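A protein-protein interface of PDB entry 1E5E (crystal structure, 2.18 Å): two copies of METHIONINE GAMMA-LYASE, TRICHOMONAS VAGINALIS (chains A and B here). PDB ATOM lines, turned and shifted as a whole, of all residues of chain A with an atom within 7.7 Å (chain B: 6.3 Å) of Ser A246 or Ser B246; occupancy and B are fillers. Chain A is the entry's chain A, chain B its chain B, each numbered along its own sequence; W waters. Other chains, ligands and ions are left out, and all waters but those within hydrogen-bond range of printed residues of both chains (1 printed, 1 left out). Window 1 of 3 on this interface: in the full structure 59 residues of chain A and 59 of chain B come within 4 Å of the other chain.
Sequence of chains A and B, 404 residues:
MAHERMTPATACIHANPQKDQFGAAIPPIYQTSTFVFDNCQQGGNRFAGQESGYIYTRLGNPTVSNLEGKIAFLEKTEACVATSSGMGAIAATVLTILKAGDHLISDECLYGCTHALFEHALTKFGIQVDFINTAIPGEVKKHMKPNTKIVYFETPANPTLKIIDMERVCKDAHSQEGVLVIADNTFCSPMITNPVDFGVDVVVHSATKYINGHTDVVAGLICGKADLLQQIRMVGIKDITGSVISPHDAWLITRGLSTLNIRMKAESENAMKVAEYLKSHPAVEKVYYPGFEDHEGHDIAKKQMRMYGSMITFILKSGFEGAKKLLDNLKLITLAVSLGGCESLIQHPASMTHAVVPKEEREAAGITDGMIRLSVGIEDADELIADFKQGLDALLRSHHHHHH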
ATOM      1  N   ILE A  29      -2.525   6.303  -8.537  1.00  0.00           N
ATOM      2  CA  ILE A  29      -2.180   7.649  -8.960  1.00  0.00           C
ATOM      3  C   ILE A  29      -0.707   7.835  -9.272  1.00  0.00           C
ATOM      4  O   ILE A  29       0.078   7.824  -8.310  1.00  0.00           O
ATOM      5  CB  ILE A  29      -2.591   8.607  -7.798  1.00  0.00           C
ATOM      6  CG1 ILE A  29      -4.033   8.364  -7.346  1.00  0.00           C
ATOM      7  CG2 ILE A  29      -2.418  10.058  -8.185  1.00  0.00           C
ATOM      8  CD1 ILE A  29      -4.482   9.157  -6.142  1.00  0.00           C
ATOM      9  N   TYR A  30      -0.294   8.064 -10.525  1.00  0.00           N
ATOM     10  CA  TYR A  30       1.130   8.277 -10.794  1.00  0.00           C
ATOM     11  C   TYR A  30       1.539   9.691 -10.424  1.00  0.00           C
ATOM     12  O   TYR A  30       1.876  10.451 -11.333  1.00  0.00           O
ATOM     13  CB  TYR A  30       1.445   7.915 -12.265  1.00  0.00           C
ATOM     14  CG  TYR A  30       1.621   6.402 -12.344  1.00  0.00           C
ATOM     15  CD1 TYR A  30       2.871   5.814 -12.174  1.00  0.00           C
ATOM     16  CD2 TYR A  30       0.520   5.600 -12.495  1.00  0.00           C
ATOM     17  CE1 TYR A  30       2.987   4.453 -12.159  1.00  0.00           C
ATOM     18  CE2 TYR A  30       0.605   4.230 -12.496  1.00  0.00           C
ATOM     19  CZ  TYR A  30       1.863   3.665 -12.338  1.00  0.00           C
ATOM     20  OH  TYR A  30       1.965   2.302 -12.331  1.00  0.00           O
ATOM     21  N   GLN A  31       1.638  10.049  -9.148  1.00  0.00           N
ATOM     22  CA  GLN A  31       2.043  11.382  -8.675  1.00  0.00           C
ATOM     23  C   GLN A  31       3.564  11.344  -8.552  1.00  0.00           C
ATOM     24  O   GLN A  31       4.216  11.182  -7.532  1.00  0.00           O
ATOM     25  CB  GLN A  31       1.416  11.736  -7.327  1.00  0.00           C
ATOM     26  CG  GLN A  31       1.623  13.125  -6.735  1.00  0.00           C
ATOM     27  CD  GLN A  31       0.755  14.121  -7.457  1.00  0.00           C
ATOM     28  OE1 GLN A  31      -0.380  13.824  -7.801  1.00  0.00           O
ATOM     29  NE2 GLN A  31       1.228  15.305  -7.793  1.00  0.00           N
ATOM     30  N   THR A  57       6.453  13.734 -16.584  1.00  0.00           N
ATOM     31  CA  THR A  57       5.028  14.097 -16.571  1.00  0.00           C
ATOM     32  C   THR A  57       4.565  15.261 -17.409  1.00  0.00           C
ATOM     33  O   THR A  57       3.414  15.211 -17.896  1.00  0.00           O
ATOM     34  CB  THR A  57       4.565  14.189 -15.086  1.00  0.00           C
ATOM     35  OG1 THR A  57       4.664  12.817 -14.632  1.00  0.00           O
ATOM     36  CG2 THR A  57       3.153  14.725 -14.906  1.00  0.00           C
ATOM     37  N   ASN A  61       1.984  10.739 -18.786  1.00  0.00           N
ATOM     38  CA  ASN A  61       1.938  10.103 -17.465  1.00  0.00           C
ATOM     39  C   ASN A  61       0.836   9.056 -17.541  1.00  0.00           C
ATOM     40  O   ASN A  61      -0.194   9.251 -18.207  1.00  0.00           O
ATOM     41  CB  ASN A  61       1.648  11.226 -16.455  1.00  0.00           C
ATOM     42  CG  ASN A  61       1.432  10.673 -15.050  1.00  0.00           C
ATOM     43  OD1 ASN A  61       0.395  10.069 -14.773  1.00  0.00           O
ATOM     44  ND2 ASN A  61       2.375  10.857 -14.128  1.00  0.00           N
ATOM     45  N   THR A  63      -1.399   7.807 -15.422  1.00  0.00           N
ATOM     46  CA  THR A  63      -2.754   8.144 -14.941  1.00  0.00           C
ATOM     47  C   THR A  63      -3.419   9.081 -15.950  1.00  0.00           C
ATOM     48  O   THR A  63      -4.618   9.045 -16.174  1.00  0.00           O
ATOM     49  CB  THR A  63      -2.648   8.822 -13.563  1.00  0.00           C
ATOM     50  OG1 THR A  63      -2.115   7.877 -12.622  1.00  0.00           O
ATOM     51  CG2 THR A  63      -3.949   9.423 -13.064  1.00  0.00           C
ATOM     52  N   VAL A  64      -2.641  10.010 -16.527  1.00  0.00           N
ATOM     53  CA  VAL A  64      -3.218  10.989 -17.459  1.00  0.00           C
ATOM     54  C   VAL A  64      -3.628  10.255 -18.750  1.00  0.00           C
ATOM     55  O   VAL A  64      -4.740  10.522 -19.180  1.00  0.00           O
ATOM     56  CB  VAL A  64      -2.289  12.203 -17.721  1.00  0.00           C
ATOM     57  CG1 VAL A  64      -2.838  13.169 -18.755  1.00  0.00           C
ATOM     58  CG2 VAL A  64      -2.037  12.975 -16.404  1.00  0.00           C
ATOM     59  N   LEU A  67      -7.171   8.545 -18.291  1.00  0.00           N
ATOM     60  CA  LEU A  67      -8.269   9.473 -18.560  1.00  0.00           C
ATOM     61  C   LEU A  67      -8.382   9.806 -20.061  1.00  0.00           C
ATOM     62  O   LEU A  67      -9.459   9.849 -20.623  1.00  0.00           O
ATOM     63  CB  LEU A  67      -7.932  10.825 -17.887  1.00  0.00           C
ATOM     64  CG  LEU A  67      -8.930  11.961 -18.156  1.00  0.00           C
ATOM     65  CD1 LEU A  67     -10.313  11.453 -17.692  1.00  0.00           C
ATOM     66  CD2 LEU A  67      -8.472  13.232 -17.435  1.00  0.00           C
ATOM     67  N   THR A  83      -5.319  18.677 -20.145  1.00  0.00           N
ATOM     68  CA  THR A  83      -4.581  19.856 -19.775  1.00  0.00           C
ATOM     69  C   THR A  83      -5.062  20.307 -18.387  1.00  0.00           C
ATOM     70  O   THR A  83      -5.984  19.710 -17.806  1.00  0.00           O
ATOM     71  CB  THR A  83      -4.762  21.057 -20.722  1.00  0.00           C
ATOM     72  OG1 THR A  83      -6.127  21.447 -20.588  1.00  0.00           O
ATOM     73  CG2 THR A  83      -4.441  20.733 -22.181  1.00  0.00           C
ATOM     74  N   SER A  84      -4.365  21.334 -17.881  1.00  0.00           N
ATOM     75  CA  SER A  84      -4.697  21.810 -16.553  1.00  0.00           C
ATOM     76  C   SER A  84      -5.766  22.896 -16.552  1.00  0.00           C
ATOM     77  O   SER A  84      -6.017  23.453 -15.484  1.00  0.00           O
ATOM     78  CB  SER A  84      -3.450  22.171 -15.720  1.00  0.00           C
ATOM     79  OG  SER A  84      -2.882  23.378 -16.158  1.00  0.00           O
ATOM     80  N   ASP A 216     -14.440  20.398  -8.183  1.00  0.00           N
ATOM     81  CA  ASP A 216     -13.232  20.430  -7.367  1.00  0.00           C
ATOM     82  C   ASP A 216     -11.971  20.314  -8.187  1.00  0.00           C
ATOM     83  O   ASP A 216     -10.860  20.226  -7.600  1.00  0.00           O
ATOM     84  CB  ASP A 216     -13.304  19.334  -6.285  1.00  0.00           C
ATOM     85  CG  ASP A 216     -13.549  17.949  -6.844  1.00  0.00           C
ATOM     86  OD1 ASP A 216     -13.549  17.771  -8.105  1.00  0.00           O
ATOM     87  OD2 ASP A 216     -13.792  17.033  -6.022  1.00  0.00           O
ATOM     88  N   VAL A 217     -12.084  20.281  -9.515  1.00  0.00           N
ATOM     89  CA  VAL A 217     -10.915  20.162 -10.365  1.00  0.00           C
ATOM     90  C   VAL A 217     -10.977  21.160 -11.515  1.00  0.00           C
ATOM     91  O   VAL A 217     -12.027  21.250 -12.150  1.00  0.00           O
ATOM     92  CB  VAL A 217     -10.763  18.748 -10.960  1.00  0.00           C
ATOM     93  CG1 VAL A 217      -9.723  18.698 -12.104  1.00  0.00           C
ATOM     94  CG2 VAL A 217     -10.282  17.801  -9.863  1.00  0.00           C
ATOM     95  N   VAL A 218      -9.862  21.792 -11.842  1.00  0.00           N
ATOM     96  CA  VAL A 218      -9.805  22.653 -13.027  1.00  0.00           C
ATOM     97  C   VAL A 218      -8.962  21.878 -14.038  1.00  0.00           C
ATOM     98  O   VAL A 218      -7.850  21.521 -13.679  1.00  0.00           O
ATOM     99  CB  VAL A 218      -9.199  24.051 -12.804  1.00  0.00           C
ATOM    100  CG1 VAL A 218      -9.089  24.783 -14.145  1.00  0.00           C
ATOM    101  CG2 VAL A 218     -10.137  24.802 -11.855  1.00  0.00           C
ATOM    102  N   ALA A 219      -9.497  21.600 -15.217  1.00  0.00           N
ATOM    103  CA  ALA A 219      -8.791  20.822 -16.201  1.00  0.00           C
ATOM    104  C   ALA A 219      -9.481  20.944 -17.551  1.00  0.00           C
ATOM    105  O   ALA A 219     -10.627  21.389 -17.650  1.00  0.00           O
ATOM    106  CB  ALA A 219      -8.859  19.340 -15.777  1.00  0.00           C
ATOM    107  N   SER A 243       0.623  23.731 -19.869  1.00  0.00           N
ATOM    108  CA  SER A 243      -0.612  23.444 -19.147  1.00  0.00           C
ATOM    109  C   SER A 243      -0.643  21.946 -18.832  1.00  0.00           C
ATOM    110  O   SER A 243      -1.310  21.131 -19.468  1.00  0.00           O
ATOM    111  CB  SER A 243      -1.829  23.866 -19.976  1.00  0.00           C
ATOM    112  OG  SER A 243      -3.018  23.702 -19.220  1.00  0.00           O
ATOM    113  N   VAL A 244       0.142  21.596 -17.814  1.00  0.00           N
ATOM    114  CA  VAL A 244       0.362  20.212 -17.465  1.00  0.00           C
ATOM    115  C   VAL A 244      -0.592  19.777 -16.355  1.00  0.00           C
ATOM    116  O   VAL A 244      -0.397  20.214 -15.210  1.00  0.00           O
ATOM    117  CB  VAL A 244       1.830  19.966 -17.028  1.00  0.00           C
ATOM    118  CG1 VAL A 244       1.987  18.492 -16.695  1.00  0.00           C
ATOM    119  CG2 VAL A 244       2.774  20.373 -18.176  1.00  0.00           C
ATOM    120  N   ILE A 245      -1.468  18.840 -16.693  1.00  0.00           N
ATOM    121  CA  ILE A 245      -2.419  18.422 -15.658  1.00  0.00           C
ATOM    122  C   ILE A 245      -1.714  17.631 -14.560  1.00  0.00           C
ATOM    123  O   ILE A 245      -0.866  16.774 -14.826  1.00  0.00           O
ATOM    124  CB  ILE A 245      -3.590  17.622 -16.222  1.00  0.00           C
ATOM    125  CG1 ILE A 245      -4.718  17.449 -15.167  1.00  0.00           C
ATOM    126  CG2 ILE A 245      -3.158  16.246 -16.698  1.00  0.00           C
ATOM    127  CD1 ILE A 245      -5.933  16.715 -15.756  1.00  0.00           C
ATOM    128  N   SER A 246      -2.152  17.808 -13.337  1.00  0.00           N
ATOM    129  CA  SER A 246      -1.705  17.033 -12.185  1.00  0.00           C
ATOM    130  C   SER A 246      -2.287  15.624 -12.304  1.00  0.00           C
ATOM    131  O   SER A 246      -3.520  15.486 -12.382  1.00  0.00           O
ATOM    132  CB  SER A 246      -2.284  17.600 -10.880  1.00  0.00           C
ATOM    133  OG  SER A 246      -2.185  16.623  -9.825  1.00  0.00           O
ATOM    134  N   PRO A 247      -1.478  14.599 -12.105  1.00  0.00           N
ATOM    135  CA  PRO A 247      -1.931  13.227 -12.110  1.00  0.00           C
ATOM    136  C   PRO A 247      -2.992  12.972 -11.054  1.00  0.00           C
ATOM    137  O   PRO A 247      -3.950  12.224 -11.269  1.00  0.00           O
ATOM    138  CB  PRO A 247      -0.658  12.387 -11.847  1.00  0.00           C
ATOM    139  CG  PRO A 247       0.419  13.299 -12.376  1.00  0.00           C
ATOM    140  CD  PRO A 247       0.004  14.697 -11.923  1.00  0.00           C
ATOM    141  N   HIS A 248      -2.914  13.660  -9.923  1.00  0.00           N
ATOM    142  CA  HIS A 248      -3.912  13.533  -8.870  1.00  0.00           C
ATOM    143  C   HIS A 248      -5.243  14.073  -9.379  1.00  0.00           C
ATOM    144  O   HIS A 248      -6.260  13.449  -9.174  1.00  0.00           O
ATOM    145  CB  HIS A 248      -3.413  14.282  -7.635  1.00  0.00           C
ATOM    146  CG  HIS A 248      -4.508  14.607  -6.660  1.00  0.00           C
ATOM    147  ND1 HIS A 248      -5.254  15.780  -6.829  1.00  0.00           N
ATOM    148  CD2 HIS A 248      -5.022  13.962  -5.605  1.00  0.00           C
ATOM    149  CE1 HIS A 248      -6.160  15.837  -5.877  1.00  0.00           C
ATOM    150  NE2 HIS A 248      -6.033  14.743  -5.118  1.00  0.00           N
ATOM    151  N   ASP A 249      -5.281  15.156 -10.113  1.00  0.00           N
ATOM    152  CA  ASP A 249      -6.493  15.742 -10.659  1.00  0.00           C
ATOM    153  C   ASP A 249      -7.017  14.887 -11.802  1.00  0.00           C
ATOM    154  O   ASP A 249      -8.223  14.636 -11.865  1.00  0.00           O
ATOM    155  CB  ASP A 249      -6.268  17.169 -11.145  1.00  0.00           C
ATOM    156  CG  ASP A 249      -6.167  18.221 -10.080  1.00  0.00           C
ATOM    157  OD1 ASP A 249      -5.866  17.930  -8.916  1.00  0.00           O
ATOM    158  OD2 ASP A 249      -6.182  19.428 -10.434  1.00  0.00           O
ATOM    159  N   ALA A 250      -6.121  14.369 -12.650  1.00  0.00           N
ATOM    160  CA  ALA A 250      -6.599  13.477 -13.703  1.00  0.00           C
ATOM    161  C   ALA A 250      -7.312  12.278 -13.078  1.00  0.00           C
ATOM    162  O   ALA A 250      -8.352  11.827 -13.587  1.00  0.00           O
ATOM    163  CB  ALA A 250      -5.490  12.930 -14.576  1.00  0.00           C
ATOM    164  N   TRP A 251      -6.697  11.706 -12.022  1.00  0.00           N
ATOM    165  CA  TRP A 251      -7.342  10.573 -11.354  1.00  0.00           C
ATOM    166  C   TRP A 251      -8.711  10.942 -10.805  1.00  0.00           C
ATOM    167  O   TRP A 251      -9.627  10.118 -10.894  1.00  0.00           O
ATOM    168  CB  TRP A 251      -6.423  10.122 -10.189  1.00  0.00           C
ATOM    169  CG  TRP A 251      -6.860   8.915  -9.414  1.00  0.00           C
ATOM    170  CD1 TRP A 251      -6.474   7.628  -9.675  1.00  0.00           C
ATOM    171  CD2 TRP A 251      -7.641   8.860  -8.214  1.00  0.00           C
ATOM    172  NE1 TRP A 251      -6.990   6.797  -8.695  1.00  0.00           N
ATOM    173  CE2 TRP A 251      -7.678   7.533  -7.781  1.00  0.00           C
ATOM    174  CE3 TRP A 251      -8.263   9.835  -7.436  1.00  0.00           C
ATOM    175  CZ2 TRP A 251      -8.388   7.114  -6.658  1.00  0.00           C
ATOM    176  CZ3 TRP A 251      -8.954   9.464  -6.284  1.00  0.00           C
ATOM    177  CH2 TRP A 251      -9.007   8.108  -5.920  1.00  0.00           C
ATOM    178  N   LEU A 252      -8.886  12.140 -10.235  1.00  0.00           N
ATOM    179  CA  LEU A 252     -10.163  12.616  -9.741  1.00  0.00           C
ATOM    180  C   LEU A 252     -11.193  12.786 -10.859  1.00  0.00           C
ATOM    181  O   LEU A 252     -12.404  12.506 -10.695  1.00  0.00           O
ATOM    182  CB  LEU A 252     -10.011  13.934  -8.958  1.00  0.00           C
ATOM    183  CG  LEU A 252      -9.432  13.945  -7.556  1.00  0.00           C
ATOM    184  CD1 LEU A 252      -9.339  15.403  -7.023  1.00  0.00           C
ATOM    185  CD2 LEU A 252     -10.313  13.162  -6.554  1.00  0.00           C
ATOM    186  N   ILE A 253     -10.770  13.174 -12.038  1.00  0.00           N
ATOM    187  CA  ILE A 253     -11.613  13.367 -13.224  1.00  0.00           C
ATOM    188  C   ILE A 253     -12.089  11.986 -13.672  1.00  0.00           C
ATOM    189  O   ILE A 253     -13.288  11.800 -13.858  1.00  0.00           O
ATOM    190  CB  ILE A 253     -10.938  14.095 -14.390  1.00  0.00           C
ATOM    191  CG1 ILE A 253     -10.563  15.545 -13.960  1.00  0.00           C
ATOM    192  CG2 ILE A 253     -11.897  14.146 -15.616  1.00  0.00           C
ATOM    193  CD1 ILE A 253      -9.612  16.198 -14.974  1.00  0.00           C
ATOM    194  N   GLN B  31      -9.223  22.264  -2.681  1.00  0.00           N
ATOM    195  CA  GLN B  31      -9.480  21.522  -3.927  1.00  0.00           C
ATOM    196  C   GLN B  31     -10.916  21.826  -4.344  1.00  0.00           C
ATOM    197  O   GLN B  31     -11.832  21.068  -4.072  1.00  0.00           O
ATOM    198  CB  GLN B  31      -9.270  20.014  -3.738  1.00  0.00           C
ATOM    199  CG  GLN B  31      -9.348  19.163  -5.015  1.00  0.00           C
ATOM    200  CD  GLN B  31      -8.049  19.309  -5.797  1.00  0.00           C
ATOM    201  OE1 GLN B  31      -6.940  19.390  -5.219  1.00  0.00           O
ATOM    202  NE2 GLN B  31      -8.085  19.396  -7.103  1.00  0.00           N
ATOM    203  N   THR B  57     -10.780  28.937  -9.485  1.00  0.00           N
ATOM    204  CA  THR B  57      -9.394  28.466  -9.378  1.00  0.00           C
ATOM    205  C   THR B  57      -8.480  28.817 -10.506  1.00  0.00           C
ATOM    206  O   THR B  57      -7.305  29.047 -10.170  1.00  0.00           O
ATOM    207  CB  THR B  57      -9.385  27.019  -8.847  1.00  0.00           C
ATOM    208  OG1 THR B  57      -9.798  27.177  -7.466  1.00  0.00           O
ATOM    209  CG2 THR B  57      -7.999  26.397  -8.967  1.00  0.00           C
ATOM    210  N   THR B  63      -5.016  28.127  -1.265  1.00  0.00           N
ATOM    211  CA  THR B  63      -3.880  27.238  -1.064  1.00  0.00           C
ATOM    212  C   THR B  63      -2.737  27.695  -1.988  1.00  0.00           C
ATOM    213  O   THR B  63      -1.572  27.695  -1.591  1.00  0.00           O
ATOM    214  CB  THR B  63      -4.299  25.795  -1.411  1.00  0.00           C
ATOM    215  OG1 THR B  63      -5.282  25.417  -0.439  1.00  0.00           O
ATOM    216  CG2 THR B  63      -3.127  24.812  -1.430  1.00  0.00           C
ATOM    217  N   VAL B  64      -3.081  28.058  -3.229  1.00  0.00           N
ATOM    218  CA  VAL B  64      -2.036  28.502  -4.170  1.00  0.00           C
ATOM    219  C   VAL B  64      -1.420  29.821  -3.705  1.00  0.00           C
ATOM    220  O   VAL B  64      -0.188  29.978  -3.735  1.00  0.00           O
ATOM    221  CB  VAL B  64      -2.603  28.597  -5.592  1.00  0.00           C
ATOM    222  CG1 VAL B  64      -1.567  29.093  -6.591  1.00  0.00           C
ATOM    223  CG2 VAL B  64      -3.152  27.238  -6.047  1.00  0.00           C
ATOM    224  N   SER B  84       1.373  25.399 -13.542  1.00  0.00           N
ATOM    225  CA  SER B  84       1.375  23.949 -13.557  1.00  0.00           C
ATOM    226  C   SER B  84       2.605  23.378 -14.232  1.00  0.00           C
ATOM    227  O   SER B  84       2.710  22.160 -14.278  1.00  0.00           O
ATOM    228  CB  SER B  84       0.078  23.333 -14.098  1.00  0.00           C
ATOM    229  OG  SER B  84      -0.134  23.565 -15.445  1.00  0.00           O
ATOM    230  N   VAL B 244      -2.803  26.291 -15.008  1.00  0.00           N
ATOM    231  CA  VAL B 244      -3.347  26.454 -13.672  1.00  0.00           C
ATOM    232  C   VAL B 244      -2.918  25.363 -12.722  1.00  0.00           C
ATOM    233  O   VAL B 244      -3.247  24.188 -12.943  1.00  0.00           O
ATOM    234  CB  VAL B 244      -4.886  26.493 -13.784  1.00  0.00           C
ATOM    235  CG1 VAL B 244      -5.484  26.641 -12.386  1.00  0.00           C
ATOM    236  CG2 VAL B 244      -5.270  27.641 -14.725  1.00  0.00           C
ATOM    237  N   ILE B 245      -2.142  25.722 -11.696  1.00  0.00           N
ATOM    238  CA  ILE B 245      -1.702  24.573 -10.856  1.00  0.00           C
ATOM    239  C   ILE B 245      -2.871  23.996 -10.066  1.00  0.00           C
ATOM    240  O   ILE B 245      -3.777  24.672  -9.553  1.00  0.00           O
ATOM    241  CB  ILE B 245      -0.593  25.071  -9.926  1.00  0.00           C
ATOM    242  CG1 ILE B 245       0.050  23.987  -9.051  1.00  0.00           C
ATOM    243  CG2 ILE B 245      -1.105  26.194  -9.023  1.00  0.00           C
ATOM    244  CD1 ILE B 245       1.329  24.592  -8.412  1.00  0.00           C
ATOM    245  N   SER B 246      -2.879  22.702  -9.861  1.00  0.00           N
ATOM    246  CA  SER B 246      -3.765  22.036  -8.944  1.00  0.00           C
ATOM    247  C   SER B 246      -3.409  22.479  -7.503  1.00  0.00           C
ATOM    248  O   SER B 246      -2.261  22.447  -7.021  1.00  0.00           O
ATOM    249  CB  SER B 246      -3.464  20.527  -8.988  1.00  0.00           C
ATOM    250  OG  SER B 246      -4.161  19.926  -7.901  1.00  0.00           O
ATOM    251  N   PRO B 247      -4.421  22.890  -6.761  1.00  0.00           N
ATOM    252  CA  PRO B 247      -4.281  23.258  -5.358  1.00  0.00           C
ATOM    253  C   PRO B 247      -3.669  22.097  -4.571  1.00  0.00           C
ATOM    254  O   PRO B 247      -2.900  22.304  -3.638  1.00  0.00           O
ATOM    255  CB  PRO B 247      -5.712  23.528  -4.920  1.00  0.00           C
ATOM    256  CG  PRO B 247      -6.422  23.893  -6.198  1.00  0.00           C
ATOM    257  CD  PRO B 247      -5.838  22.971  -7.232  1.00  0.00           C
ATOM    258  N   HIS B 248      -4.027  20.848  -4.817  1.00  0.00           N
ATOM    259  CA  HIS B 248      -3.390  19.672  -4.256  1.00  0.00           C
ATOM    260  C   HIS B 248      -1.861  19.675  -4.508  1.00  0.00           C
ATOM    261  O   HIS B 248      -1.097  19.402  -3.588  1.00  0.00           O
ATOM    262  CB  HIS B 248      -4.000  18.396  -4.850  1.00  0.00           C
ATOM    263  CG  HIS B 248      -3.262  17.155  -4.417  1.00  0.00           C
ATOM    264  ND1 HIS B 248      -2.286  16.555  -5.240  1.00  0.00           N
ATOM    265  CD2 HIS B 248      -3.337  16.437  -3.280  1.00  0.00           C
ATOM    266  CE1 HIS B 248      -1.829  15.500  -4.596  1.00  0.00           C
ATOM    267  NE2 HIS B 248      -2.435  15.404  -3.425  1.00  0.00           N
ATOM    268  N   ASP B 249      -1.422  19.960  -5.728  1.00  0.00           N
ATOM    269  CA  ASP B 249      -0.006  20.040  -6.026  1.00  0.00           C
ATOM    270  C   ASP B 249       0.646  21.251  -5.337  1.00  0.00           C
ATOM    271  O   ASP B 249       1.746  21.120  -4.794  1.00  0.00           O
ATOM    272  CB  ASP B 249       0.282  20.126  -7.515  1.00  0.00           C
ATOM    273  CG  ASP B 249       0.085  18.793  -8.217  1.00  0.00           C
ATOM    274  OD1 ASP B 249      -0.619  17.935  -7.693  1.00  0.00           O
ATOM    275  OD2 ASP B 249       0.553  18.639  -9.360  1.00  0.00           O
ATOM    276  N   ALA B 250      -0.029  22.393  -5.270  1.00  0.00           N
ATOM    277  CA  ALA B 250       0.519  23.554  -4.563  1.00  0.00           C
ATOM    278  C   ALA B 250       0.745  23.205  -3.099  1.00  0.00           C
ATOM    279  O   ALA B 250       1.794  23.571  -2.576  1.00  0.00           O
ATOM    280  CB  ALA B 250      -0.387  24.782  -4.624  1.00  0.00           C
ATOM    281  N   TRP B 251      -0.214  22.524  -2.460  1.00  0.00           N
ATOM    282  CA  TRP B 251      -0.110  22.102  -1.070  1.00  0.00           C
ATOM    283  C   TRP B 251       1.052  21.086  -0.959  1.00  0.00           C
ATOM    284  O   TRP B 251       1.781  21.281   0.023  1.00  0.00           O
ATOM    285  CB  TRP B 251      -1.398  21.426  -0.614  1.00  0.00           C
ATOM    286  CG  TRP B 251      -1.475  20.960   0.805  1.00  0.00           C
ATOM    287  CD1 TRP B 251      -2.026  21.647   1.854  1.00  0.00           C
ATOM    288  CD2 TRP B 251      -1.134  19.656   1.318  1.00  0.00           C
ATOM    289  NE1 TRP B 251      -1.915  20.897   3.017  1.00  0.00           N
ATOM    290  CE2 TRP B 251      -1.406  19.664   2.682  1.00  0.00           C
ATOM    291  CE3 TRP B 251      -0.591  18.524   0.735  1.00  0.00           C
ATOM    292  CZ2 TRP B 251      -1.172  18.554   3.505  1.00  0.00           C
ATOM    293  CZ3 TRP B 251      -0.296  17.412   1.548  1.00  0.00           C
ATOM    294  CH2 TRP B 251      -0.599  17.445   2.921  1.00  0.00           C
HETATM  295  O   HOH W   1       1.322  19.614 -13.100  1.00  0.00           O
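The backbone NH of Val B244 sits at hydrogen-bond distance from the side-chain hydroxyl of Ser A84 (3.1 Å). OG of Ser B84 is in hydrogen-bond range of OG of Ser A84 (2.8 Å). The side-chain hydroxyl of Ser A246 lies within hydrogen-bond range of the side-chain carboxylate of Asp B249 (3.0 Å). N of Val A244 is in hydrogen-bond range of OG of Ser B84 (3.1 Å). The backbone carbonyl oxygen of Asp A216 is in hydrogen-bond range of the side-chain amide nitrogen of Gln B31, at 2.9 Å. The side-chain carboxylate (OD1) of Asp A249 is in hydrogen-bond range of the side-chain amide nitrogen (NE2) of Gln B31, at 3.2 Å. A ring nitrogen (ND1) of His A248 sits close to a ring nitrogen (ND1) of His B248. NE2 of Gln A31 sits at hydrogen-bond distance from OD1 of Asp B249, at 3.2 Å. OG of Ser B246 lies within hydrogen-bond range of OD1 of Asp A249, 2.8 Å away.
Hydrophobic or aromatic side chains of chain A within 4 Å of the printed part of chain B: Val A217, Val A218, Val A244 and His A248. Printed residues of chain B that touch a printed residue of chain A: Gln B31, Thr B57, Ser B84, Val B244, Ser B246, His B248 and Asp B249. Hydrophobic or aromatic side chains of chain B within 4 Å of the printed part of chain A: Val B244 and His B248. Among the printed residues, no Asp or Glu carboxylate lies within 4 Å of a Lys or Arg side-chain nitrogen of the other chain.
Among the printed residues, merely in contact across the chains: Gln A31 with His B248, Val A217 with Gln B31, Val A218 with Thr B57, Ser A243 with Ser B84, Ser A246 with Ser B246 and His A248 with Gln B31.
Ser B84 touches its own counterpart, Ser A84. Ser A246 touches its own counterpart, Ser B246. Ser A246 touches Asp B249, and with the chains exchanged Asp A249 touches Ser B246. His A248 touches its own counterpart, His B248. Positions printed for both chains: 31, 57, 63, 64, 84, 244, 245, 246, 247, 248, 249, 250 and 251. Of the 15 pairs that touch across the chains among the printed residues, 11 have their exchanged pair printed and touching as well.
Tyr A30 touches none of the printed residues of chain B. Printed residues of chain B within 4 Å of Gln A31: His B248 (3.9 Å) and Asp B249 (3.2 Å). Of the printed residues of chain B, Ser A84 touches Ser B84 (2.8 Å) and Val B244 (3.1 Å). Of the printed residues of chain B, Ser A246 touches Ser B246 and Asp B249. Leu A252 touches none of the printed residues of chain B. Of the printed residues of chain A, Thr B57 touches Val A218. Ser B246 touches just these residues of chain A: Ser A246 (3.7 Å) and Asp A249 (2.8 Å). No residue of chain A comes within 4 Å of Pro B247. The nearest residue of chain B that does not touch Ser A246 is His B248 (4.6 Å).
ND1 of His A248 sits at hydrogen-bond distance from OD1 of Asp A249 (3.1 Å). OE1 of Gln B31 sits close to N of His B248, 3.3 Å away. The side-chain hydroxyl (OG) of Ser B246 sits close to the backbone NH (N) of His B248 (3.2 Å). N of Asp B249 lies within hydrogen-bond range of OG of Ser B246. The side-chain hydroxyl of Ser A246 sits at hydrogen-bond distance from the backbone NH of Asp A249, 3.4 Å away. A ring nitrogen (ND1) of His B248 is in hydrogen-bond range of the side-chain carboxylate (OD1) of Asp B249 (3.3 Å).
Water W1 bridges O of Val A244 (2.8 Å) and O of Ser B84 (3.1 Å).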
